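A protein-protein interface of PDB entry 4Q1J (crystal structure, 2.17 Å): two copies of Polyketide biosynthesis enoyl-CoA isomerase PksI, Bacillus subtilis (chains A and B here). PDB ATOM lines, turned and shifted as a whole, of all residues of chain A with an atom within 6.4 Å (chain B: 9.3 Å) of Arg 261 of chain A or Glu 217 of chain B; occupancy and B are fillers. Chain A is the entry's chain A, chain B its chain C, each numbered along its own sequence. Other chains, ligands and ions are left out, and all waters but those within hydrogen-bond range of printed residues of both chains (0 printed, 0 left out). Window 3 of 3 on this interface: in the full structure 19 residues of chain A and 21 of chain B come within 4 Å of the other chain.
Glu 217 of chain B touches just one residue of chain A: Arg 261. No residue of chain B comes within 4 Å of Ser 260 of chain A. No residue of chain B comes within 4 Å of Leu 265 of chain A. Printed residues of chain B within 4 Å of Asn 180 of chain A: Leu 211 (3.4 Å), Glu 214 (2.8 Å), Leu 215 (3.3 Å) and Lys 218 (2.8 Å). Of the printed residues of chain A, Glu 214 of chain B touches Asn 180 (2.8 Å). Of the printed residues of chain A, Pro 219 of chain B touches Glu 257 and Arg 261. Of the printed residues of chain A, Leu 215 of chain B touches Asn 180. Printed residues of chain B within 4 Å of Glu 257 of chain A: Pro 219. The nearest residue of chain B that does not touch Arg 261 of chain A is Lys 218 of chain B (4.3 Å).
The backbone carbonyl oxygen (O) of Glu 214 of chain B is in hydrogen-bond range of the side-chain amino group (NZ) of Lys 218 of chain B. The side-chain amino group (NZ) of Lys 70 of chain B lies within hydrogen-bond range of the backbone carbonyl oxygen (O) of Lys 218 of chain B, 2.9 Å away. The guanidinium group of Arg 261 of chain A is in salt-bridge range of the side-chain carboxylate of Glu 257 of chain A (2.8 Å).
Along chain A the printed residues that touch a printed residue of chain B span positions 151 to 261. Of the 20 printed residues of chain B, 7 touch a printed residue of chain A. Hydrophobic or aromatic side chains of chain B that line the printed part of chain A: Leu 211, Leu 215 and Pro 219. Among the printed residues, 10 pairs touch across the chains. Among the printed residues, no Asp or Glu carboxylate lies within 4 Å of a Lys or Arg side-chain nitrogen of the other chain.
No position is printed for both chains.
CG of Lys 218 of chain B touches O of Met 151 of chain A, at 3.5 Å. Ser 222 of chain B touches Met 151 of chain A (CB to CE, 3.8 Å). Leu 211 of chain B touches Asn 180 of chain A. Glu 257 of chain A touches Pro 219 of chain B. Arg 261 of chain A touches Pro 219 of chain B.
The side-chain amino group (NZ) of Lys 218 of chain B lies within hydrogen-bond range of the backbone carbonyl oxygen (O) of Asn 180 of chain A (2.8 Å). NH2 of Arg 261 of chain A is in hydrogen-bond range of O of Glu 217 of chain B. The side-chain amide nitrogen (ND2) of Asn 180 of chain A sits close to the backbone NH (N) of Leu 215 of chain B, 3.3 Å away. O of Gly 154 of chain A lies within hydrogen-bond range of OG of Ser 222 of chain B, at 2.8 Å. The side-chain carboxylate (OE1) of Glu 214 of chain B lies close to the side-chain amide oxygen (OD1) of Asn 180 of chain A, 2.8 Å away.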
ATOM      1  N   MET A 151      11.173  -0.207  -4.093  1.00  0.00           N
ATOM      2  CA  MET A 151      11.327   0.171  -2.691  1.00  0.00           C
ATOM      3  C   MET A 151      11.390   1.694  -2.422  1.00  0.00           C
ATOM      4  O   MET A 151      11.018   2.157  -1.334  1.00  0.00           O
ATOM      5  CB  MET A 151      12.530  -0.631  -2.050  1.00  0.00           C
ATOM      6  CG  MET A 151      12.202  -2.126  -1.841  1.00  0.00           C
ATOM      7  SD  MET A 151      11.503  -2.344  -0.171  1.00  0.00           S
ATOM      8  CE  MET A 151      10.168  -3.404  -0.460  1.00  0.00           C
ATOM      9  N   LYS A 152      11.795   2.506  -3.392  1.00  0.00           N
ATOM     10  CA  LYS A 152      11.695   4.003  -3.237  1.00  0.00           C
ATOM     11  C   LYS A 152      10.258   4.423  -2.858  1.00  0.00           C
ATOM     12  O   LYS A 152      10.012   5.418  -2.178  1.00  0.00           O
ATOM     13  CB  LYS A 152      12.070   4.678  -4.575  1.00  0.00           C
ATOM     14  CG  LYS A 152      12.108   6.200  -4.586  1.00  0.00           C
ATOM     15  CD  LYS A 152      12.405   6.797  -5.975  1.00  0.00           C
ATOM     16  CE  LYS A 152      11.198   6.697  -6.934  1.00  0.00           C
ATOM     17  NZ  LYS A 152      11.296   7.598  -8.136  1.00  0.00           N
ATOM     18  N   TYR A 153       9.299   3.673  -3.357  1.00  0.00           N
ATOM     19  CA  TYR A 153       7.869   3.996  -3.210  1.00  0.00           C
ATOM     20  C   TYR A 153       7.266   3.296  -2.008  1.00  0.00           C
ATOM     21  O   TYR A 153       6.064   3.410  -1.762  1.00  0.00           O
ATOM     22  CB  TYR A 153       7.095   3.512  -4.437  1.00  0.00           C
ATOM     23  CG  TYR A 153       7.433   4.283  -5.677  1.00  0.00           C
ATOM     24  CD1 TYR A 153       7.272   5.684  -5.723  1.00  0.00           C
ATOM     25  CD2 TYR A 153       7.935   3.634  -6.798  1.00  0.00           C
ATOM     26  CE1 TYR A 153       7.599   6.410  -6.889  1.00  0.00           C
ATOM     27  CE2 TYR A 153       8.220   4.309  -7.976  1.00  0.00           C
ATOM     28  CZ  TYR A 153       8.078   5.682  -8.033  1.00  0.00           C
ATOM     29  OH  TYR A 153       8.447   6.340  -9.180  1.00  0.00           O
ATOM     30  N   GLY A 154       8.092   2.546  -1.284  1.00  0.00           N
ATOM     31  CA  GLY A 154       7.588   1.675  -0.230  1.00  0.00           C
ATOM     32  C   GLY A 154       7.083   0.304  -0.674  1.00  0.00           C
ATOM     33  O   GLY A 154       6.815  -0.522   0.179  1.00  0.00           O
ATOM     34  N   PHE A 155       6.999   0.023  -1.977  1.00  0.00           N
ATOM     35  CA  PHE A 155       6.599  -1.289  -2.444  1.00  0.00           C
ATOM     36  C   PHE A 155       7.770  -2.272  -2.284  1.00  0.00           C
ATOM     37  O   PHE A 155       8.945  -1.926  -2.547  1.00  0.00           O
ATOM     38  CB  PHE A 155       6.399  -1.329  -3.969  1.00  0.00           C
ATOM     39  CG  PHE A 155       5.269  -0.555  -4.514  1.00  0.00           C
ATOM     40  CD1 PHE A 155       3.938  -0.922  -4.243  1.00  0.00           C
ATOM     41  CD2 PHE A 155       5.520   0.390  -5.502  1.00  0.00           C
ATOM     42  CE1 PHE A 155       2.836  -0.263  -4.867  1.00  0.00           C
ATOM     43  CE2 PHE A 155       4.460   1.061  -6.125  1.00  0.00           C
ATOM     44  CZ  PHE A 155       3.105   0.738  -5.809  1.00  0.00           C
ATOM     45  N   ASN A 180      17.767  -1.203  -1.644  1.00  0.00           N
ATOM     46  CA  ASN A 180      17.934   0.220  -1.542  1.00  0.00           C
ATOM     47  C   ASN A 180      17.282   0.986  -2.730  1.00  0.00           C
ATOM     48  O   ASN A 180      17.204   2.223  -2.683  1.00  0.00           O
ATOM     49  CB  ASN A 180      19.421   0.568  -1.380  1.00  0.00           C
ATOM     50  CG  ASN A 180      19.635   2.026  -0.944  1.00  0.00           C
ATOM     51  OD1 ASN A 180      20.516   2.742  -1.479  1.00  0.00           O
ATOM     52  ND2 ASN A 180      18.803   2.493  -0.016  1.00  0.00           N
ATOM     53  N   GLU A 256      -1.134   3.937   3.270  1.00  0.00           N
ATOM     54  CA  GLU A 256      -1.291   5.292   2.750  1.00  0.00           C
ATOM     55  C   GLU A 256       0.044   5.875   2.303  1.00  0.00           C
ATOM     56  O   GLU A 256       0.095   6.613   1.298  1.00  0.00           O
ATOM     57  CB  GLU A 256      -1.905   6.225   3.819  1.00  0.00           C
ATOM     58  CG  GLU A 256      -2.332   7.593   3.291  1.00  0.00           C
ATOM     59  CD  GLU A 256      -3.486   7.515   2.294  1.00  0.00           C
ATOM     60  OE1 GLU A 256      -4.255   6.523   2.311  1.00  0.00           O
ATOM     61  OE2 GLU A 256      -3.636   8.454   1.487  1.00  0.00           O
ATOM     62  N   GLU A 257       1.113   5.566   3.053  1.00  0.00           N
ATOM     63  CA  GLU A 257       2.407   6.158   2.750  1.00  0.00           C
ATOM     64  C   GLU A 257       3.006   5.789   1.364  1.00  0.00           C
ATOM     65  O   GLU A 257       3.874   6.517   0.834  1.00  0.00           O
ATOM     66  CB  GLU A 257       3.405   5.958   3.904  1.00  0.00           C
ATOM     67  CG  GLU A 257       4.193   4.664   3.917  1.00  0.00           C
ATOM     68  CD  GLU A 257       5.416   4.803   4.854  1.00  0.00           C
ATOM     69  OE1 GLU A 257       5.391   4.178   5.953  1.00  0.00           O
ATOM     70  OE2 GLU A 257       6.378   5.575   4.511  1.00  0.00           O
ATOM     71  N   VAL A 258       2.552   4.677   0.794  1.00  0.00           N
ATOM     72  CA  VAL A 258       2.991   4.243  -0.535  1.00  0.00           C
ATOM     73  C   VAL A 258       2.356   5.210  -1.562  1.00  0.00           C
ATOM     74  O   VAL A 258       3.041   5.781  -2.449  1.00  0.00           O
ATOM     75  CB  VAL A 258       2.624   2.750  -0.788  1.00  0.00           C
ATOM     76  CG1 VAL A 258       2.833   2.393  -2.259  1.00  0.00           C
ATOM     77  CG2 VAL A 258       3.402   1.788   0.138  1.00  0.00           C
ATOM     78  N   LYS A 259       1.045   5.404  -1.416  1.00  0.00           N
ATOM     79  CA  LYS A 259       0.318   6.444  -2.173  1.00  0.00           C
ATOM     80  C   LYS A 259       1.068   7.783  -2.088  1.00  0.00           C
ATOM     81  O   LYS A 259       1.360   8.400  -3.100  1.00  0.00           O
ATOM     82  CB  LYS A 259      -1.144   6.558  -1.675  1.00  0.00           C
ATOM     83  CG  LYS A 259      -1.982   7.647  -2.334  1.00  0.00           C
ATOM     84  CD  LYS A 259      -3.439   7.528  -1.924  1.00  0.00           C
ATOM     85  CE  LYS A 259      -4.063   8.904  -1.903  1.00  0.00           C
ATOM     86  NZ  LYS A 259      -5.539   8.841  -1.683  1.00  0.00           N
ATOM     87  N   SER A 260       1.432   8.209  -0.881  1.00  0.00           N
ATOM     88  CA  SER A 260       2.172   9.482  -0.716  1.00  0.00           C
ATOM     89  C   SER A 260       3.518   9.450  -1.422  1.00  0.00           C
ATOM     90  O   SER A 260       3.868  10.432  -2.041  1.00  0.00           O
ATOM     91  CB  SER A 260       2.362   9.893   0.770  1.00  0.00           C
ATOM     92  OG  SER A 260       1.155   9.765   1.497  1.00  0.00           O
ATOM     93  N   ARG A 261       4.277   8.343  -1.333  1.00  0.00           N
ATOM     94  CA  ARG A 261       5.582   8.259  -2.065  1.00  0.00           C
ATOM     95  C   ARG A 261       5.391   8.284  -3.608  1.00  0.00           C
ATOM     96  O   ARG A 261       6.086   9.016  -4.318  1.00  0.00           O
ATOM     97  CB  ARG A 261       6.370   7.022  -1.643  1.00  0.00           C
ATOM     98  CG  ARG A 261       6.938   7.082  -0.234  1.00  0.00           C
ATOM     99  CD  ARG A 261       7.035   5.699   0.385  1.00  0.00           C
ATOM    100  NE  ARG A 261       7.376   5.781   1.799  1.00  0.00           N
ATOM    101  CZ  ARG A 261       8.611   6.019   2.227  1.00  0.00           C
ATOM    102  NH1 ARG A 261       9.579   6.172   1.340  1.00  0.00           N
ATOM    103  NH2 ARG A 261       8.889   6.103   3.520  1.00  0.00           N
ATOM    104  N   ILE A 262       4.434   7.499  -4.116  1.00  0.00           N
ATOM    105  CA  ILE A 262       4.078   7.586  -5.539  1.00  0.00           C
ATOM    106  C   ILE A 262       3.709   8.992  -5.953  1.00  0.00           C
ATOM    107  O   ILE A 262       4.210   9.474  -6.953  1.00  0.00           O
ATOM    108  CB  ILE A 262       2.878   6.685  -5.964  1.00  0.00           C
ATOM    109  CG1 ILE A 262       3.226   5.206  -5.768  1.00  0.00           C
ATOM    110  CG2 ILE A 262       2.530   6.984  -7.418  1.00  0.00           C
ATOM    111  CD1 ILE A 262       2.054   4.241  -5.795  1.00  0.00           C
ATOM    112  N   LYS A 263       2.797   9.635  -5.230  1.00  0.00           N
ATOM    113  CA  LYS A 263       2.375  10.964  -5.662  1.00  0.00           C
ATOM    114  C   LYS A 263       3.600  11.883  -5.520  1.00  0.00           C
ATOM    115  O   LYS A 263       3.754  12.810  -6.287  1.00  0.00           O
ATOM    116  CB  LYS A 263       1.148  11.544  -4.904  1.00  0.00           C
ATOM    117  CG  LYS A 263      -0.170  10.766  -4.944  1.00  0.00           C
ATOM    118  CD  LYS A 263      -1.438  11.606  -5.154  1.00  0.00           C
ATOM    119  CE  LYS A 263      -1.324  13.110  -4.838  1.00  0.00           C
ATOM    120  NZ  LYS A 263      -2.114  13.697  -3.699  1.00  0.00           N
ATOM    121  N   GLY A 264       4.477  11.616  -4.561  1.00  0.00           N
ATOM    122  CA  GLY A 264       5.541  12.598  -4.252  1.00  0.00           C
ATOM    123  C   GLY A 264       6.860  12.365  -4.992  1.00  0.00           C
ATOM    124  O   GLY A 264       7.609  13.327  -5.300  1.00  0.00           O
ATOM    125  N   LEU A 265       7.175  11.117  -5.296  1.00  0.00           N
ATOM    126  CA  LEU A 265       8.468  10.781  -5.872  1.00  0.00           C
ATOM    127  C   LEU A 265       8.571  10.435  -7.380  1.00  0.00           C
ATOM    128  O   LEU A 265       9.664  10.281  -7.876  1.00  0.00           O
ATOM    129  CB  LEU A 265       9.182   9.753  -4.997  1.00  0.00           C
ATOM    130  CG  LEU A 265       9.205  10.090  -3.518  1.00  0.00           C
ATOM    131  CD1 LEU A 265       9.762   8.990  -2.679  1.00  0.00           C
ATOM    132  CD2 LEU A 265       9.981  11.326  -3.235  1.00  0.00           C
ATOM    133  N   TYR A 266       7.448  10.335  -8.093  1.00  0.00           N
ATOM    134  CA  TYR A 266       7.435  10.247  -9.559  1.00  0.00           C
ATOM    135  C   TYR A 266       6.345   9.364 -10.135  1.00  0.00           C
ATOM    136  O   TYR A 266       5.687   8.692  -9.437  1.00  0.00           O
ATOM    137  CB  TYR A 266       8.711   9.651 -10.047  1.00  0.00           C
ATOM    138  CG  TYR A 266       9.617  10.459 -10.892  1.00  0.00           C
ATOM    139  CD1 TYR A 266      10.506  11.317 -10.324  1.00  0.00           C
ATOM    140  CD2 TYR A 266       9.706  10.240 -12.249  1.00  0.00           C
ATOM    141  CE1 TYR A 266      11.404  12.005 -11.075  1.00  0.00           C
ATOM    142  CE2 TYR A 266      10.609  10.920 -13.021  1.00  0.00           C
ATOM    143  CZ  TYR A 266      11.451  11.813 -12.421  1.00  0.00           C
ATOM    144  OH  TYR A 266      12.370  12.522 -13.154  1.00  0.00           O
ATOM    145  N   SER B  32      18.463   9.203  12.948  1.00  0.00           N
ATOM    146  CA  SER B  32      17.299   8.753  13.674  1.00  0.00           C
ATOM    147  C   SER B  32      17.295   7.260  13.881  1.00  0.00           C
ATOM    148  O   SER B  32      17.133   6.807  15.005  1.00  0.00           O
ATOM    149  CB  SER B  32      15.975   9.097  12.920  1.00  0.00           C
ATOM    150  OG  SER B  32      15.685  10.508  12.962  1.00  0.00           O
ATOM    151  N   ALA B  33      17.452   6.475  12.816  1.00  0.00           N
ATOM    152  CA  ALA B  33      17.220   5.032  12.907  1.00  0.00           C
ATOM    153  C   ALA B  33      18.400   4.153  12.439  1.00  0.00           C
ATOM    154  O   ALA B  33      18.150   3.067  11.894  1.00  0.00           O
ATOM    155  CB  ALA B  33      15.969   4.696  12.043  1.00  0.00           C
ATOM    156  N   ILE B  34      19.643   4.645  12.534  1.00  0.00           N
ATOM    157  CA  ILE B  34      20.782   3.876  12.105  1.00  0.00           C
ATOM    158  C   ILE B  34      21.554   3.555  13.357  1.00  0.00           C
ATOM    159  O   ILE B  34      21.711   4.410  14.213  1.00  0.00           O
ATOM    160  CB  ILE B  34      21.666   4.675  11.143  1.00  0.00           C
ATOM    161  CG1 ILE B  34      20.971   4.888   9.779  1.00  0.00           C
ATOM    162  CG2 ILE B  34      22.971   3.948  10.830  1.00  0.00           C
ATOM    163  CD1 ILE B  34      21.601   6.044   9.005  1.00  0.00           C
ATOM    164  N   LYS B  70      16.493   0.820  11.478  1.00  0.00           N
ATOM    165  CA  LYS B  70      16.194   0.358  10.136  1.00  0.00           C
ATOM    166  C   LYS B  70      17.436  -0.242   9.404  1.00  0.00           C
ATOM    167  O   LYS B  70      17.257  -0.948   8.406  1.00  0.00           O
ATOM    168  CB  LYS B  70      15.716   1.548   9.328  1.00  0.00           C
ATOM    169  CG  LYS B  70      14.250   1.843   9.524  1.00  0.00           C
ATOM    170  CD  LYS B  70      13.959   3.197   8.898  1.00  0.00           C
ATOM    171  CE  LYS B  70      12.435   3.490   8.869  1.00  0.00           C
ATOM    172  NZ  LYS B  70      12.172   4.724   8.069  1.00  0.00           N
ATOM    173  N   ALA B  71      18.653   0.136   9.815  1.00  0.00           N
ATOM    174  CA  ALA B  71      19.866  -0.326   9.168  1.00  0.00           C
ATOM    175  C   ALA B  71      20.941  -0.373  10.244  1.00  0.00           C
ATOM    176  O   ALA B  71      20.976   0.499  11.090  1.00  0.00           O
ATOM    177  CB  ALA B  71      20.303   0.628   8.044  1.00  0.00           C
ATOM    178  N   VAL B 209      27.633   5.165   5.684  1.00  0.00           N
ATOM    179  CA  VAL B 209      26.718   5.973   6.477  1.00  0.00           C
ATOM    180  C   VAL B 209      25.657   6.479   5.459  1.00  0.00           C
ATOM    181  O   VAL B 209      24.502   6.343   5.705  1.00  0.00           O
ATOM    182  CB  VAL B 209      27.453   7.145   7.213  1.00  0.00           C
ATOM    183  CG1 VAL B 209      26.486   8.194   7.700  1.00  0.00           C
ATOM    184  CG2 VAL B 209      28.304   6.643   8.402  1.00  0.00           C
ATOM    185  N   GLU B 210      26.116   6.945   4.300  1.00  0.00           N
ATOM    186  CA  GLU B 210      25.279   7.410   3.197  1.00  0.00           C
ATOM    187  C   GLU B 210      24.330   6.360   2.744  1.00  0.00           C
ATOM    188  O   GLU B 210      23.114   6.630   2.608  1.00  0.00           O
ATOM    189  CB  GLU B 210      26.130   7.877   2.006  1.00  0.00           C
ATOM    190  CG  GLU B 210      26.627   9.288   2.239  1.00  0.00           C
ATOM    191  CD  GLU B 210      27.577   9.833   1.174  1.00  0.00           C
ATOM    192  OE1 GLU B 210      27.616   9.320   0.039  1.00  0.00           O
ATOM    193  OE2 GLU B 210      28.290  10.816   1.476  1.00  0.00           O
ATOM    194  N   LEU B 211      24.873   5.179   2.455  1.00  0.00           N
ATOM    195  CA  LEU B 211      24.037   4.031   2.136  1.00  0.00           C
ATOM    196  C   LEU B 211      23.039   3.721   3.241  1.00  0.00           C
ATOM    197  O   LEU B 211      21.811   3.533   2.959  1.00  0.00           O
ATOM    198  CB  LEU B 211      24.931   2.826   1.880  1.00  0.00           C
ATOM    199  CG  LEU B 211      24.326   1.549   1.321  1.00  0.00           C
ATOM    200  CD1 LEU B 211      23.236   1.778   0.270  1.00  0.00           C
ATOM    201  CD2 LEU B 211      25.504   0.793   0.728  1.00  0.00           C
ATOM    202  N   ALA B 212      23.523   3.650   4.505  1.00  0.00           N
ATOM    203  CA  ALA B 212      22.549   3.487   5.644  1.00  0.00           C
ATOM    204  C   ALA B 212      21.427   4.561   5.649  1.00  0.00           C
ATOM    205  O   ALA B 212      20.207   4.204   5.835  1.00  0.00           O
ATOM    206  CB  ALA B 212      23.279   3.482   6.971  1.00  0.00           C
ATOM    207  N   GLN B 213      21.771   5.845   5.399  1.00  0.00           N
ATOM    208  CA  GLN B 213      20.688   6.879   5.353  1.00  0.00           C
ATOM    209  C   GLN B 213      19.691   6.614   4.230  1.00  0.00           C
ATOM    210  O   GLN B 213      18.495   6.878   4.393  1.00  0.00           O
ATOM    211  CB  GLN B 213      21.190   8.320   5.198  1.00  0.00           C
ATOM    212  CG  GLN B 213      22.089   8.793   6.323  1.00  0.00           C
ATOM    213  CD  GLN B 213      22.905  10.033   5.944  1.00  0.00           C
ATOM    214  OE1 GLN B 213      23.769   9.996   5.066  1.00  0.00           O
ATOM    215  NE2 GLN B 213      22.671  11.110   6.638  1.00  0.00           N
ATOM    216  N   GLU B 214      20.160   6.094   3.100  1.00  0.00           N
ATOM    217  CA  GLU B 214      19.266   5.817   1.960  1.00  0.00           C
ATOM    218  C   GLU B 214      18.365   4.666   2.284  1.00  0.00           C
ATOM    219  O   GLU B 214      17.208   4.673   1.884  1.00  0.00           O
ATOM    220  CB  GLU B 214      20.017   5.534   0.655  1.00  0.00           C
ATOM    221  CG  GLU B 214      20.509   6.797  -0.053  1.00  0.00           C
ATOM    222  CD  GLU B 214      21.515   6.451  -1.133  1.00  0.00           C
ATOM    223  OE1 GLU B 214      21.399   5.385  -1.740  1.00  0.00           O
ATOM    224  OE2 GLU B 214      22.462   7.196  -1.375  1.00  0.00           O
ATOM    225  N   LEU B 215      18.888   3.710   3.049  1.00  0.00           N
ATOM    226  CA  LEU B 215      18.104   2.554   3.479  1.00  0.00           C
ATOM    227  C   LEU B 215      17.044   2.998   4.475  1.00  0.00           C
ATOM    228  O   LEU B 215      15.933   2.470   4.455  1.00  0.00           O
ATOM    229  CB  LEU B 215      18.980   1.445   4.122  1.00  0.00           C
ATOM    230  CG  LEU B 215      19.871   0.639   3.147  1.00  0.00           C
ATOM    231  CD1 LEU B 215      20.901  -0.275   3.868  1.00  0.00           C
ATOM    232  CD2 LEU B 215      18.960  -0.122   2.199  1.00  0.00           C
ATOM    233  N   ALA B 216      17.374   4.018   5.281  1.00  0.00           N
ATOM    234  CA  ALA B 216      16.526   4.431   6.375  1.00  0.00           C
ATOM    235  C   ALA B 216      15.382   5.303   5.820  1.00  0.00           C
ATOM    236  O   ALA B 216      14.501   5.635   6.552  1.00  0.00           O
ATOM    237  CB  ALA B 216      17.312   5.184   7.443  1.00  0.00           C
ATOM    238  N   GLU B 217      15.397   5.628   4.526  1.00  0.00           N
ATOM    239  CA  GLU B 217      14.273   6.294   3.871  1.00  0.00           C
ATOM    240  C   GLU B 217      13.049   5.411   3.646  1.00  0.00           C
ATOM    241  O   GLU B 217      11.955   5.891   3.350  1.00  0.00           O
ATOM    242  CB  GLU B 217      14.750   6.820   2.535  1.00  0.00           C
ATOM    243  CG  GLU B 217      15.615   8.058   2.701  1.00  0.00           C
ATOM    244  CD  GLU B 217      16.229   8.457   1.372  1.00  0.00           C
ATOM    245  OE1 GLU B 217      15.851   7.891   0.310  1.00  0.00           O
ATOM    246  OE2 GLU B 217      17.060   9.362   1.366  1.00  0.00           O
ATOM    247  N   LYS B 218      13.256   4.121   3.713  1.00  0.00           N
ATOM    248  CA  LYS B 218      12.209   3.139   3.453  1.00  0.00           C
ATOM    249  C   LYS B 218      11.407   2.809   4.756  1.00  0.00           C
ATOM    250  O   LYS B 218      11.948   2.858   5.868  1.00  0.00           O
ATOM    251  CB  LYS B 218      12.901   1.861   2.909  1.00  0.00           C
ATOM    252  CG  LYS B 218      13.223   1.843   1.403  1.00  0.00           C
ATOM    253  CD  LYS B 218      14.190   2.928   0.971  1.00  0.00           C
ATOM    254  CE  LYS B 218      14.968   2.584  -0.282  1.00  0.00           C
ATOM    255  NZ  LYS B 218      16.091   3.578  -0.447  1.00  0.00           N
ATOM    256  N   PRO B 219      10.159   2.395   4.619  1.00  0.00           N
ATOM    257  CA  PRO B 219       9.463   1.909   5.819  1.00  0.00           C
ATOM    258  C   PRO B 219      10.082   0.641   6.368  1.00  0.00           C
ATOM    259  O   PRO B 219      10.374  -0.314   5.590  1.00  0.00           O
ATOM    260  CB  PRO B 219       8.038   1.575   5.327  1.00  0.00           C
ATOM    261  CG  PRO B 219       8.035   1.836   3.859  1.00  0.00           C
ATOM    262  CD  PRO B 219       9.374   2.271   3.372  1.00  0.00           C
ATOM    263  N   ARG B 220      10.210   0.592   7.703  1.00  0.00           N
ATOM    264  CA  ARG B 220      10.879  -0.554   8.381  1.00  0.00           C
ATOM    265  C   ARG B 220      10.205  -1.867   8.005  1.00  0.00           C
ATOM    266  O   ARG B 220      10.877  -2.880   7.791  1.00  0.00           O
ATOM    267  CB  ARG B 220      10.850  -0.422   9.896  1.00  0.00           C
ATOM    268  CG  ARG B 220      11.827  -1.373  10.567  1.00  0.00           C
ATOM    269  CD  ARG B 220      11.640  -1.231  12.033  1.00  0.00           C
ATOM    270  NE  ARG B 220      12.631  -2.001  12.726  1.00  0.00           N
ATOM    271  CZ  ARG B 220      12.492  -3.284  13.080  1.00  0.00           C
ATOM    272  NH1 ARG B 220      11.407  -3.953  12.791  1.00  0.00           N
ATOM    273  NH2 ARG B 220      13.449  -3.879  13.742  1.00  0.00           N
ATOM    274  N   ASN B 221       8.883  -1.822   7.847  1.00  0.00           N
ATOM    275  CA  ASN B 221       8.148  -3.017   7.507  1.00  0.00           C
ATOM    276  C   ASN B 221       8.515  -3.528   6.113  1.00  0.00           C
ATOM    277  O   ASN B 221       8.606  -4.727   5.891  1.00  0.00           O
ATOM    278  CB  ASN B 221       6.630  -2.802   7.617  1.00  0.00           C
ATOM    279  CG  ASN B 221       5.859  -4.072   7.326  1.00  0.00           C
ATOM    280  OD1 ASN B 221       5.979  -5.031   8.048  1.00  0.00           O
ATOM    281  ND2 ASN B 221       5.133  -4.100   6.229  1.00  0.00           N
ATOM    282  N   SER B 222       8.743  -2.626   5.172  1.00  0.00           N
ATOM    283  CA  SER B 222       9.096  -3.049   3.810  1.00  0.00           C
ATOM    284  C   SER B 222      10.527  -3.623   3.801  1.00  0.00           C
ATOM    285  O   SER B 222      10.775  -4.594   3.095  1.00  0.00           O
ATOM    286  CB  SER B 222       8.999  -1.902   2.811  1.00  0.00           C
ATOM    287  OG  SER B 222       7.664  -1.438   2.704  1.00  0.00           O
ATOM    288  N   LEU B 223      11.418  -3.048   4.605  1.00  0.00           N
ATOM    289  CA  LEU B 223      12.809  -3.524   4.695  1.00  0.00           C
ATOM    290  C   LEU B 223      12.944  -4.924   5.300  1.00  0.00           C
ATOM    291  O   LEU B 223      13.754  -5.754   4.852  1.00  0.00           O
ATOM    292  CB  LEU B 223      13.645  -2.546   5.518  1.00  0.00           C
ATOM    293  CG  LEU B 223      14.042  -1.170   4.943  1.00  0.00           C
ATOM    294  CD1 LEU B 223      14.738  -0.446   6.100  1.00  0.00           C
ATOM    295  CD2 LEU B 223      14.998  -1.247   3.718  1.00  0.00           C
